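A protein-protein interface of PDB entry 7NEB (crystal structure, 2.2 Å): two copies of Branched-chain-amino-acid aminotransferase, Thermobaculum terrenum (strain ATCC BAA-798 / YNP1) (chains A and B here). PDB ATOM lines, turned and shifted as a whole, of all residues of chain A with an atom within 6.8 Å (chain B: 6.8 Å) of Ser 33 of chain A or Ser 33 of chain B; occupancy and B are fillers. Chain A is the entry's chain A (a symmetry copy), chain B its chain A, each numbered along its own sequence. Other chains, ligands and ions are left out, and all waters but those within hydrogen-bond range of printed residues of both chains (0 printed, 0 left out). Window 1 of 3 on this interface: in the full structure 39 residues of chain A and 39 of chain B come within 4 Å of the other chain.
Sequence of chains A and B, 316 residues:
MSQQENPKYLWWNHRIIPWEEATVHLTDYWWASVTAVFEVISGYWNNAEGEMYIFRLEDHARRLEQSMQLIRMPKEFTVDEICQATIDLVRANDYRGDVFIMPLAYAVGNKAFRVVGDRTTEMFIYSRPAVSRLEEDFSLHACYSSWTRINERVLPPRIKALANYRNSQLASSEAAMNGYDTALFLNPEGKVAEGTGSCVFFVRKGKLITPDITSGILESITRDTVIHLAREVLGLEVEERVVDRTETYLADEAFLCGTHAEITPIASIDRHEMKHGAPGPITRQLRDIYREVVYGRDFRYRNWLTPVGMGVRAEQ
The backbone carbonyl oxygen of Trp 30 of chain B is in hydrogen-bond range of the side-chain hydroxyl of Ser 33 of chain B (2.6 Å).
The backbone carbonyl oxygen (O) of Ala 36 of chain B is in hydrogen-bond range of the backbone NH (N) of Leu 162 of chain B, at 3.1 Å.
O of Trp 30 of chain A sits at hydrogen-bond distance from OG of Ser 33 of chain A.
The backbone NH of Leu 162 of chain A lies within hydrogen-bond range of the backbone carbonyl oxygen of Ala 36 of chain A.
Of the printed residues of chain B, Trp 31 of chain A touches Leu 162 (3.5 Å).
Printed residues of chain B within 4 Å of Ser 33 of chain A: Trp 30 (3.7 Å), Ser 33 (3.4 Å) and Leu 162 (3.8 Å).
Of the printed residues of chain B, Val 34 of chain A touches Leu 162 and Arg 166.
Val 37 of chain A touches none of the printed residues of chain B.
Ser 33 of chain B touches three residues of chain A.
Ala 36 of chain B touches none of the printed residues of chain A.
Of the printed residues of chain A, Leu 104 of chain B touches Trp 30 (3.8 Å).
Among the printed residues, pairs that only touch across the chains: Tyr 29 of chain A with Trp 30 of chain B, Trp 30 of chain A with Tyr 29 of chain B, Trp 30 of chain A with Ser 33 of chain B, Trp 30 of chain A with Leu 104 of chain B, Trp 30 of chain A with Tyr 106 of chain B, Trp 30 of chain A with Leu 162 of chain B, Trp 31 of chain A with Leu 162 of chain B, Ser 33 of chain A with Trp 30 of chain B, Ser 33 of chain A with Ser 33 of chain B, Ser 33 of chain A with Leu 162 of chain B, Val 34 of chain A with Leu 162 of chain B, Leu 104 of chain A with Trp 30 of chain B, Tyr 106 of chain A with Trp 30 of chain B, Leu 162 of chain A with Trp 30 of chain B, Leu 162 of chain A with Trp 31 of chain B, Leu 162 of chain A with Ser 33 of chain B, Leu 162 of chain A with Val 34 of chain B, Ala 163 of chain A with Ala 163 of chain B, Ala 163 of chain A with Arg 166 of chain B and Arg 166 of chain A with Ala 163 of chain B.
The guanidinium group (NE) of Arg 166 of chain A sits close to the backbone carbonyl oxygen (O) of Val 34 of chain B.
The backbone carbonyl oxygen of Val 34 of chain A sits close to the guanidinium group of Arg 166 of chain B (3.4 Å).
Hydrophobic or aromatic side chains of chain A that line the printed part of chain B: Tyr 29, Trp 30, Trp 31, Val 34, Leu 104, Tyr 106, Leu 162 and Ala 163.
Of the 16 printed residues of chain B, 10 touch a printed residue of chain A.
Printed residues of chain B that touch a printed residue of chain A: Tyr 29, Trp 30, Trp 31, Ser 33, Val 34, Leu 104, Tyr 106, Leu 162, Ala 163 and Arg 166.
Among the printed residues, 22 pairs touch across the chains.
Trp 30 of chain A touches Tyr 106 of chain B, and with the chains exchanged Tyr 106 of chain A touches Trp 30 of chain B.
Ser 33 of chain A touches its own counterpart, Ser 33 of chain B.
Ala 163 of chain A touches its own counterpart, Ala 163 of chain B.
Ala 163 of chain A touches Arg 166 of chain B, and with the chains exchanged Arg 166 of chain A touches Ala 163 of chain B.
Positions printed for both chains: 29, 30, 31, 32, 33, 34, 35, 36, 37, 104, 106, 107, 161, 162, 163 and 166.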
ATOM      1  N   TYR A  29      24.321  -9.408  14.728  1.00  0.00           N
ATOM      2  CA  TYR A  29      23.926 -10.669  14.009  1.00  0.00           C
ATOM      3  C   TYR A  29      24.701 -10.732  12.653  1.00  0.00           C
ATOM      4  O   TYR A  29      24.474 -11.662  11.814  1.00  0.00           O
ATOM      5  CB  TYR A  29      22.414 -10.833  13.706  1.00  0.00           C
ATOM      6  CG  TYR A  29      21.532 -10.932  14.925  1.00  0.00           C
ATOM      7  CD1 TYR A  29      21.798 -11.814  15.938  1.00  0.00           C
ATOM      8  CD2 TYR A  29      20.432 -10.122  15.068  1.00  0.00           C
ATOM      9  CE1 TYR A  29      21.037 -11.855  17.094  1.00  0.00           C
ATOM     10  CE2 TYR A  29      19.659 -10.152  16.210  1.00  0.00           C
ATOM     11  CZ  TYR A  29      19.940 -11.036  17.217  1.00  0.00           C
ATOM     12  OH  TYR A  29      19.175 -11.038  18.335  1.00  0.00           O
ATOM     13  N   TRP A  30      25.597  -9.762  12.368  1.00  0.00           N
ATOM     14  CA  TRP A  30      26.364  -9.777  11.112  1.00  0.00           C
ATOM     15  C   TRP A  30      27.298 -10.985  11.155  1.00  0.00           C
ATOM     16  O   TRP A  30      27.265 -11.693  10.179  1.00  0.00           O
ATOM     17  CB  TRP A  30      27.091  -8.487  10.843  1.00  0.00           C
ATOM     18  CG  TRP A  30      26.161  -7.381  10.542  1.00  0.00           C
ATOM     19  CD1 TRP A  30      25.723  -6.483  11.452  1.00  0.00           C
ATOM     20  CD2 TRP A  30      25.584  -6.974   9.268  1.00  0.00           C
ATOM     21  NE1 TRP A  30      24.838  -5.608  10.868  1.00  0.00           N
ATOM     22  CE2 TRP A  30      24.717  -5.891   9.538  1.00  0.00           C
ATOM     23  CE3 TRP A  30      25.650  -7.440   7.962  1.00  0.00           C
ATOM     24  CZ2 TRP A  30      24.039  -5.191   8.550  1.00  0.00           C
ATOM     25  CZ3 TRP A  30      24.989  -6.751   6.975  1.00  0.00           C
ATOM     26  CH2 TRP A  30      24.227  -5.620   7.259  1.00  0.00           C
ATOM     27  N   TRP A  31      27.949 -11.292  12.272  1.00  0.00           N
ATOM     28  CA  TRP A  31      28.750 -12.534  12.379  1.00  0.00           C
ATOM     29  C   TRP A  31      27.793 -13.730  12.325  1.00  0.00           C
ATOM     30  O   TRP A  31      28.074 -14.642  11.587  1.00  0.00           O
ATOM     31  CB  TRP A  31      29.656 -12.516  13.616  1.00  0.00           C
ATOM     32  CG  TRP A  31      30.789 -11.552  13.455  1.00  0.00           C
ATOM     33  CD1 TRP A  31      31.116 -10.484  14.240  1.00  0.00           C
ATOM     34  CD2 TRP A  31      31.767 -11.586  12.398  1.00  0.00           C
ATOM     35  NE1 TRP A  31      32.229  -9.855  13.754  1.00  0.00           N
ATOM     36  CE2 TRP A  31      32.647 -10.511  12.620  1.00  0.00           C
ATOM     37  CE3 TRP A  31      31.988 -12.439  11.310  1.00  0.00           C
ATOM     38  CZ2 TRP A  31      33.712 -10.266  11.768  1.00  0.00           C
ATOM     39  CZ3 TRP A  31      33.049 -12.198  10.476  1.00  0.00           C
ATOM     40  CH2 TRP A  31      33.875 -11.110  10.695  1.00  0.00           C
ATOM     41  N   ALA A  32      26.629 -13.666  12.961  1.00  0.00           N
ATOM     42  CA  ALA A  32      25.673 -14.802  12.981  1.00  0.00           C
ATOM     43  C   ALA A  32      25.214 -15.124  11.553  1.00  0.00           C
ATOM     44  O   ALA A  32      24.942 -16.309  11.233  1.00  0.00           O
ATOM     45  CB  ALA A  32      24.502 -14.472  13.872  1.00  0.00           C
ATOM     46  N   SER A  33      25.185 -14.124  10.684  1.00  0.00           N
ATOM     47  CA  SER A  33      24.633 -14.279   9.322  1.00  0.00           C
ATOM     48  C   SER A  33      25.525 -15.204   8.481  1.00  0.00           C
ATOM     49  O   SER A  33      24.991 -15.801   7.538  1.00  0.00           O
ATOM     50  CB  SER A  33      24.505 -12.959   8.633  1.00  0.00           C
ATOM     51  OG  SER A  33      25.788 -12.543   8.252  1.00  0.00           O
ATOM     52  N   VAL A  34      26.815 -15.302   8.817  1.00  0.00           N
ATOM     53  CA  VAL A  34      27.776 -16.244   8.155  1.00  0.00           C
ATOM     54  C   VAL A  34      27.220 -17.692   8.274  1.00  0.00           C
ATOM     55  O   VAL A  34      27.256 -18.375   7.303  1.00  0.00           O
ATOM     56  CB  VAL A  34      29.174 -16.025   8.784  1.00  0.00           C
ATOM     57  CG1 VAL A  34      30.225 -17.007   8.308  1.00  0.00           C
ATOM     58  CG2 VAL A  34      29.667 -14.575   8.523  1.00  0.00           C
ATOM     59  N   THR A  35      26.637 -18.076   9.418  1.00  0.00           N
ATOM     60  CA  THR A  35      26.163 -19.453   9.814  1.00  0.00           C
ATOM     61  C   THR A  35      24.745 -19.725   9.294  1.00  0.00           C
ATOM     62  O   THR A  35      24.279 -20.865   9.399  1.00  0.00           O
ATOM     63  CB  THR A  35      25.931 -19.532  11.338  1.00  0.00           C
ATOM     64  OG1 THR A  35      24.711 -18.837  11.814  1.00  0.00           O
ATOM     65  CG2 THR A  35      27.196 -19.070  12.035  1.00  0.00           C
ATOM     66  N   ALA A  36      24.035 -18.667   8.931  1.00  0.00           N
ATOM     67  CA  ALA A  36      22.564 -18.653   8.843  1.00  0.00           C
ATOM     68  C   ALA A  36      22.114 -19.564   7.708  1.00  0.00           C
ATOM     69  O   ALA A  36      22.739 -19.572   6.661  1.00  0.00           O
ATOM     70  CB  ALA A  36      22.065 -17.257   8.616  1.00  0.00           C
ATOM     71  N   VAL A  37      21.013 -20.231   7.930  1.00  0.00           N
ATOM     72  CA  VAL A  37      20.345 -21.090   6.957  1.00  0.00           C
ATOM     73  C   VAL A  37      18.886 -20.707   6.984  1.00  0.00           C
ATOM     74  O   VAL A  37      18.412 -20.161   7.950  1.00  0.00           O
ATOM     75  CB  VAL A  37      20.604 -22.577   7.239  1.00  0.00           C
ATOM     76  CG1 VAL A  37      22.083 -22.892   7.125  1.00  0.00           C
ATOM     77  CG2 VAL A  37      20.091 -23.034   8.542  1.00  0.00           C
ATOM     78  N   LEU A 104      14.528 -18.494   9.255  1.00  0.00           N
ATOM     79  CA  LEU A 104      15.971 -18.253   9.185  1.00  0.00           C
ATOM     80  C   LEU A 104      16.542 -18.579  10.547  1.00  0.00           C
ATOM     81  O   LEU A 104      16.067 -17.996  11.571  1.00  0.00           O
ATOM     82  CB  LEU A 104      16.164 -16.796   8.763  1.00  0.00           C
ATOM     83  CG  LEU A 104      17.591 -16.422   8.413  1.00  0.00           C
ATOM     84  CD1 LEU A 104      17.571 -15.217   7.494  1.00  0.00           C
ATOM     85  CD2 LEU A 104      18.365 -16.148   9.706  1.00  0.00           C
ATOM     86  N   TYR A 106      20.041 -19.175  12.974  1.00  0.00           N
ATOM     87  CA  TYR A 106      21.380 -18.582  13.085  1.00  0.00           C
ATOM     88  C   TYR A 106      21.890 -18.940  14.469  1.00  0.00           C
ATOM     89  O   TYR A 106      21.113 -19.084  15.435  1.00  0.00           O
ATOM     90  CB  TYR A 106      21.310 -17.072  12.778  1.00  0.00           C
ATOM     91  CG  TYR A 106      20.422 -16.260  13.714  1.00  0.00           C
ATOM     92  CD1 TYR A 106      20.914 -15.689  14.885  1.00  0.00           C
ATOM     93  CD2 TYR A 106      19.093 -16.064  13.446  1.00  0.00           C
ATOM     94  CE1 TYR A 106      20.096 -14.973  15.764  1.00  0.00           C
ATOM     95  CE2 TYR A 106      18.264 -15.375  14.331  1.00  0.00           C
ATOM     96  CZ  TYR A 106      18.744 -14.834  15.503  1.00  0.00           C
ATOM     97  OH  TYR A 106      17.913 -14.196  16.406  1.00  0.00           O
ATOM     98  N   ALA A 107      23.211 -19.014  14.571  1.00  0.00           N
ATOM     99  CA  ALA A 107      23.912 -19.342  15.815  1.00  0.00           C
ATOM    100  C   ALA A 107      24.585 -18.072  16.298  1.00  0.00           C
ATOM    101  O   ALA A 107      25.275 -17.383  15.502  1.00  0.00           O
ATOM    102  CB  ALA A 107      24.854 -20.476  15.540  1.00  0.00           C
ATOM    103  N   ALA A 161      22.334 -22.015   2.922  1.00  0.00           N
ATOM    104  CA  ALA A 161      23.028 -21.053   3.771  1.00  0.00           C
ATOM    105  C   ALA A 161      23.007 -19.736   3.020  1.00  0.00           C
ATOM    106  O   ALA A 161      23.075 -19.784   1.848  1.00  0.00           O
ATOM    107  CB  ALA A 161      24.420 -21.588   4.017  1.00  0.00           C
ATOM    108  N   LEU A 162      22.817 -18.625   3.708  1.00  0.00           N
ATOM    109  CA  LEU A 162      22.918 -17.293   3.128  1.00  0.00           C
ATOM    110  C   LEU A 162      24.281 -17.163   2.449  1.00  0.00           C
ATOM    111  O   LEU A 162      24.316 -16.574   1.412  1.00  0.00           O
ATOM    112  CB  LEU A 162      22.808 -16.244   4.239  1.00  0.00           C
ATOM    113  CG  LEU A 162      21.418 -15.899   4.764  1.00  0.00           C
ATOM    114  CD1 LEU A 162      21.528 -14.709   5.724  1.00  0.00           C
ATOM    115  CD2 LEU A 162      20.489 -15.542   3.632  1.00  0.00           C
ATOM    116  N   ALA A 163      25.357 -17.682   3.026  1.00  0.00           N
ATOM    117  CA  ALA A 163      26.697 -17.470   2.460  1.00  0.00           C
ATOM    118  C   ALA A 163      26.783 -18.037   1.027  1.00  0.00           C
ATOM    119  O   ALA A 163      27.392 -17.374   0.179  1.00  0.00           O
ATOM    120  CB  ALA A 163      27.723 -18.036   3.374  1.00  0.00           C
ATOM    121  N   ARG A 166      26.482 -15.684  -1.849  1.00  0.00           N
ATOM    122  CA  ARG A 166      27.549 -14.770  -2.340  1.00  0.00           C
ATOM    123  C   ARG A 166      27.968 -15.264  -3.742  1.00  0.00           C
ATOM    124  O   ARG A 166      28.078 -14.442  -4.662  1.00  0.00           O
ATOM    125  CB  ARG A 166      28.708 -14.742  -1.339  1.00  0.00           C
ATOM    126  CG  ARG A 166      29.928 -13.923  -1.767  1.00  0.00           C
ATOM    127  CD  ARG A 166      29.759 -12.433  -1.550  1.00  0.00           C
ATOM    128  NE  ARG A 166      28.803 -11.761  -2.452  1.00  0.00           N
ATOM    129  CZ  ARG A 166      29.074 -11.340  -3.716  1.00  0.00           C
ATOM    130  NH1 ARG A 166      30.273 -11.522  -4.267  1.00  0.00           N
ATOM    131  NH2 ARG A 166      28.130 -10.748  -4.445  1.00  0.00           N
ATOM    132  N   TYR B  29      18.247  -6.978   6.727  1.00  0.00           N
ATOM    133  CA  TYR B  29      19.685  -6.886   6.298  1.00  0.00           C
ATOM    134  C   TYR B  29      20.261  -8.334   6.170  1.00  0.00           C
ATOM    135  O   TYR B  29      21.490  -8.527   5.907  1.00  0.00           O
ATOM    136  CB  TYR B  29      20.623  -6.078   7.233  1.00  0.00           C
ATOM    137  CG  TYR B  29      20.284  -4.614   7.356  1.00  0.00           C
ATOM    138  CD1 TYR B  29      20.100  -3.822   6.253  1.00  0.00           C
ATOM    139  CD2 TYR B  29      20.134  -4.024   8.587  1.00  0.00           C
ATOM    140  CE1 TYR B  29      19.713  -2.497   6.359  1.00  0.00           C
ATOM    141  CE2 TYR B  29      19.754  -2.704   8.711  1.00  0.00           C
ATOM    142  CZ  TYR B  29      19.569  -1.925   7.601  1.00  0.00           C
ATOM    143  OH  TYR B  29      19.182  -0.635   7.748  1.00  0.00           O
ATOM    144  N   TRP B  30      19.436  -9.384   6.378  1.00  0.00           N
ATOM    145  CA  TRP B  30      19.919 -10.768   6.259  1.00  0.00           C
ATOM    146  C   TRP B  30      20.279 -11.009   4.794  1.00  0.00           C
ATOM    147  O   TRP B  30      21.371 -11.486   4.606  1.00  0.00           O
ATOM    148  CB  TRP B  30      18.949 -11.786   6.795  1.00  0.00           C
ATOM    149  CG  TRP B  30      18.817 -11.704   8.263  1.00  0.00           C
ATOM    150  CD1 TRP B  30      17.843 -11.021   8.905  1.00  0.00           C
ATOM    151  CD2 TRP B  30      19.607 -12.348   9.303  1.00  0.00           C
ATOM    152  NE1 TRP B  30      18.022 -11.106  10.266  1.00  0.00           N
ATOM    153  CE2 TRP B  30      19.101 -11.895  10.543  1.00  0.00           C
ATOM    154  CE3 TRP B  30      20.709 -13.191   9.325  1.00  0.00           C
ATOM    155  CZ2 TRP B  30      19.562 -12.352  11.770  1.00  0.00           C
ATOM    156  CZ3 TRP B  30      21.170 -13.655  10.532  1.00  0.00           C
ATOM    157  CH2 TRP B  30      20.580 -13.273  11.735  1.00  0.00           C
ATOM    158  N   TRP B  31      19.494 -10.551   3.824  1.00  0.00           N
ATOM    159  CA  TRP B  31      19.891 -10.651   2.401  1.00  0.00           C
ATOM    160  C   TRP B  31      21.102  -9.740   2.174  1.00  0.00           C
ATOM    161  O   TRP B  31      22.043 -10.195   1.571  1.00  0.00           O
ATOM    162  CB  TRP B  31      18.711 -10.362   1.465  1.00  0.00           C
ATOM    163  CG  TRP B  31      17.712 -11.476   1.479  1.00  0.00           C
ATOM    164  CD1 TRP B  31      16.384 -11.423   1.794  1.00  0.00           C
ATOM    165  CD2 TRP B  31      17.992 -12.850   1.153  1.00  0.00           C
ATOM    166  NE1 TRP B  31      15.816 -12.663   1.681  1.00  0.00           N
ATOM    167  CE2 TRP B  31      16.784 -13.558   1.291  1.00  0.00           C
ATOM    168  CE3 TRP B  31      19.141 -13.531   0.734  1.00  0.00           C
ATOM    169  CZ2 TRP B  31      16.717 -14.920   1.046  1.00  0.00           C
ATOM    170  CZ3 TRP B  31      19.067 -14.877   0.484  1.00  0.00           C
ATOM    171  CH2 TRP B  31      17.875 -15.556   0.667  1.00  0.00           C
ATOM    172  N   ALA B  32      21.148  -8.552   2.768  1.00  0.00           N
ATOM    173  CA  ALA B  32      22.274  -7.607   2.561  1.00  0.00           C
ATOM    174  C   ALA B  32      23.583  -8.236   3.054  1.00  0.00           C
ATOM    175  O   ALA B  32      24.669  -7.960   2.481  1.00  0.00           O
ATOM    176  CB  ALA B  32      21.990  -6.307   3.270  1.00  0.00           C
ATOM    177  N   SER B  33      23.500  -9.111   4.046  1.00  0.00           N
ATOM    178  CA  SER B  33      24.698  -9.679   4.698  1.00  0.00           C
ATOM    179  C   SER B  33      25.455 -10.599   3.728  1.00  0.00           C
ATOM    180  O   SER B  33      26.665 -10.759   3.927  1.00  0.00           O
ATOM    181  CB  SER B  33      24.337 -10.451   5.926  1.00  0.00           C
ATOM    182  OG  SER B  33      23.768 -11.666   5.521  1.00  0.00           O
ATOM    183  N   VAL B  34      24.760 -11.168   2.737  1.00  0.00           N
ATOM    184  CA  VAL B  34      25.384 -12.000   1.656  1.00  0.00           C
ATOM    185  C   VAL B  34      26.480 -11.156   0.944  1.00  0.00           C
ATOM    186  O   VAL B  34      27.523 -11.681   0.730  1.00  0.00           O
ATOM    187  CB  VAL B  34      24.252 -12.517   0.735  1.00  0.00           C
ATOM    188  CG1 VAL B  34      24.747 -13.265  -0.488  1.00  0.00           C
ATOM    189  CG2 VAL B  34      23.273 -13.422   1.532  1.00  0.00           C
ATOM    190  N   THR B  35      26.248  -9.859   0.696  1.00  0.00           N
ATOM    191  CA  THR B  35      27.087  -8.892  -0.101  1.00  0.00           C
ATOM    192  C   THR B  35      28.192  -8.269   0.763  1.00  0.00           C
ATOM    193  O   THR B  35      29.059  -7.578   0.217  1.00  0.00           O
ATOM    194  CB  THR B  35      26.269  -7.636  -0.470  1.00  0.00           C
ATOM    195  OG1 THR B  35      26.031  -6.700   0.655  1.00  0.00           O
ATOM    196  CG2 THR B  35      24.993  -8.087  -1.155  1.00  0.00           C
ATOM    197  N   ALA B  36      28.037  -8.360   2.075  1.00  0.00           N
ATOM    198  CA  ALA B  36      28.706  -7.474   3.047  1.00  0.00           C
ATOM    199  C   ALA B  36      30.207  -7.739   3.027  1.00  0.00           C
ATOM    200  O   ALA B  36      30.612  -8.886   2.941  1.00  0.00           O
ATOM    201  CB  ALA B  36      28.158  -7.699   4.424  1.00  0.00           C
ATOM    202  N   VAL B  37      30.961  -6.685   3.186  1.00  0.00           N
ATOM    203  CA  VAL B  37      32.417  -6.708   3.293  1.00  0.00           C
ATOM    204  C   VAL B  37      32.767  -5.851   4.483  1.00  0.00           C
ATOM    205  O   VAL B  37      32.002  -5.008   4.881  1.00  0.00           O
ATOM    206  CB  VAL B  37      33.091  -6.265   1.986  1.00  0.00           C
ATOM    207  CG1 VAL B  37      32.742  -7.216   0.857  1.00  0.00           C
ATOM    208  CG2 VAL B  37      32.775  -4.880   1.594  1.00  0.00           C
ATOM    209  N   LEU B 104      31.735  -2.028   8.139  1.00  0.00           N
ATOM    210  CA  LEU B 104      31.013  -3.077   7.415  1.00  0.00           C
ATOM    211  C   LEU B 104      30.118  -2.389   6.409  1.00  0.00           C
ATOM    212  O   LEU B 104      29.291  -1.514   6.817  1.00  0.00           O
ATOM    213  CB  LEU B 104      30.257  -3.905   8.456  1.00  0.00           C
ATOM    214  CG  LEU B 104      29.636  -5.179   7.921  1.00  0.00           C
ATOM    215  CD1 LEU B 104      29.448  -6.152   9.067  1.00  0.00           C
ATOM    216  CD2 LEU B 104      28.311  -4.836   7.234  1.00  0.00           C
ATOM    217  N   TYR B 106      27.485  -2.762   3.031  1.00  0.00           N
ATOM    218  CA  TYR B 106      26.466  -3.713   2.568  1.00  0.00           C
ATOM    219  C   TYR B 106      25.603  -2.959   1.572  1.00  0.00           C
ATOM    220  O   TYR B 106      25.411  -1.730   1.672  1.00  0.00           O
ATOM    221  CB  TYR B 106      25.714  -4.302   3.779  1.00  0.00           C
ATOM    222  CG  TYR B 106      24.969  -3.286   4.637  1.00  0.00           C
ATOM    223  CD1 TYR B 106      23.648  -2.930   4.377  1.00  0.00           C
ATOM    224  CD2 TYR B 106      25.573  -2.671   5.702  1.00  0.00           C
ATOM    225  CE1 TYR B 106      22.972  -1.973   5.141  1.00  0.00           C
ATOM    226  CE2 TYR B 106      24.915  -1.696   6.451  1.00  0.00           C
ATOM    227  CZ  TYR B 106      23.619  -1.323   6.177  1.00  0.00           C
ATOM    228  OH  TYR B 106      22.983  -0.319   6.886  1.00  0.00           O
ATOM    229  N   ALA B 107      25.028  -3.721   0.649  1.00  0.00           N
ATOM    230  CA  ALA B 107      24.154  -3.200  -0.404  1.00  0.00           C
ATOM    231  C   ALA B 107      22.742  -3.642  -0.074  1.00  0.00           C
ATOM    232  O   ALA B 107      22.511  -4.845   0.218  1.00  0.00           O
ATOM    233  CB  ALA B 107      24.665  -3.692  -1.725  1.00  0.00           C
ATOM    234  N   ALA B 161      34.738 -10.608   2.590  1.00  0.00           N
ATOM    235  CA  ALA B 161      33.284 -10.719   2.577  1.00  0.00           C
ATOM    236  C   ALA B 161      32.918 -11.602   3.753  1.00  0.00           C
ATOM    237  O   ALA B 161      33.665 -12.467   4.030  1.00  0.00           O
ATOM    238  CB  ALA B 161      32.886 -11.297   1.238  1.00  0.00           C
ATOM    239  N   LEU B 162      31.842 -11.297   4.455  1.00  0.00           N
ATOM    240  CA  LEU B 162      31.306 -12.142   5.514  1.00  0.00           C
ATOM    241  C   LEU B 162      31.078 -13.542   4.945  1.00  0.00           C
ATOM    242  O   LEU B 162      31.341 -14.465   5.655  1.00  0.00           O
ATOM    243  CB  LEU B 162      29.969 -11.571   5.994  1.00  0.00           C
ATOM    244  CG  LEU B 162      29.999 -10.393   6.963  1.00  0.00           C
ATOM    245  CD1 LEU B 162      28.573 -10.111   7.450  1.00  0.00           C
ATOM    246  CD2 LEU B 162      30.879 -10.696   8.149  1.00  0.00           C
ATOM    247  N   ALA B 163      30.593 -13.685   3.719  1.00  0.00           N
ATOM    248  CA  ALA B 163      30.250 -15.012   3.189  1.00  0.00           C
ATOM    249  C   ALA B 163      31.491 -15.931   3.164  1.00  0.00           C
ATOM    250  O   ALA B 163      31.343 -17.110   3.505  1.00  0.00           O
ATOM    251  CB  ALA B 163      29.602 -14.871   1.860  1.00  0.00           C
ATOM    252  N   ARG B 166      31.922 -18.430   5.897  1.00  0.00           N
ATOM    253  CA  ARG B 166      31.192 -19.721   6.017  1.00  0.00           C
ATOM    254  C   ARG B 166      32.226 -20.853   5.823  1.00  0.00           C
ATOM    255  O   ARG B 166      32.232 -21.805   6.615  1.00  0.00           O
ATOM    256  CB  ARG B 166      30.049 -19.768   4.999  1.00  0.00           C
ATOM    257  CG  ARG B 166      29.276 -21.087   4.935  1.00  0.00           C
ATOM    258  CD  ARG B 166      28.245 -21.234   6.037  1.00  0.00           C
ATOM    259  NE  ARG B 166      28.788 -21.442   7.394  1.00  0.00           N
ATOM    260  CZ  ARG B 166      29.204 -22.632   7.903  1.00  0.00           C
ATOM    261  NH1 ARG B 166      29.165 -23.749   7.178  1.00  0.00           N
ATOM    262  NH2 ARG B 166      29.682 -22.704   9.143  1.00  0.00           N
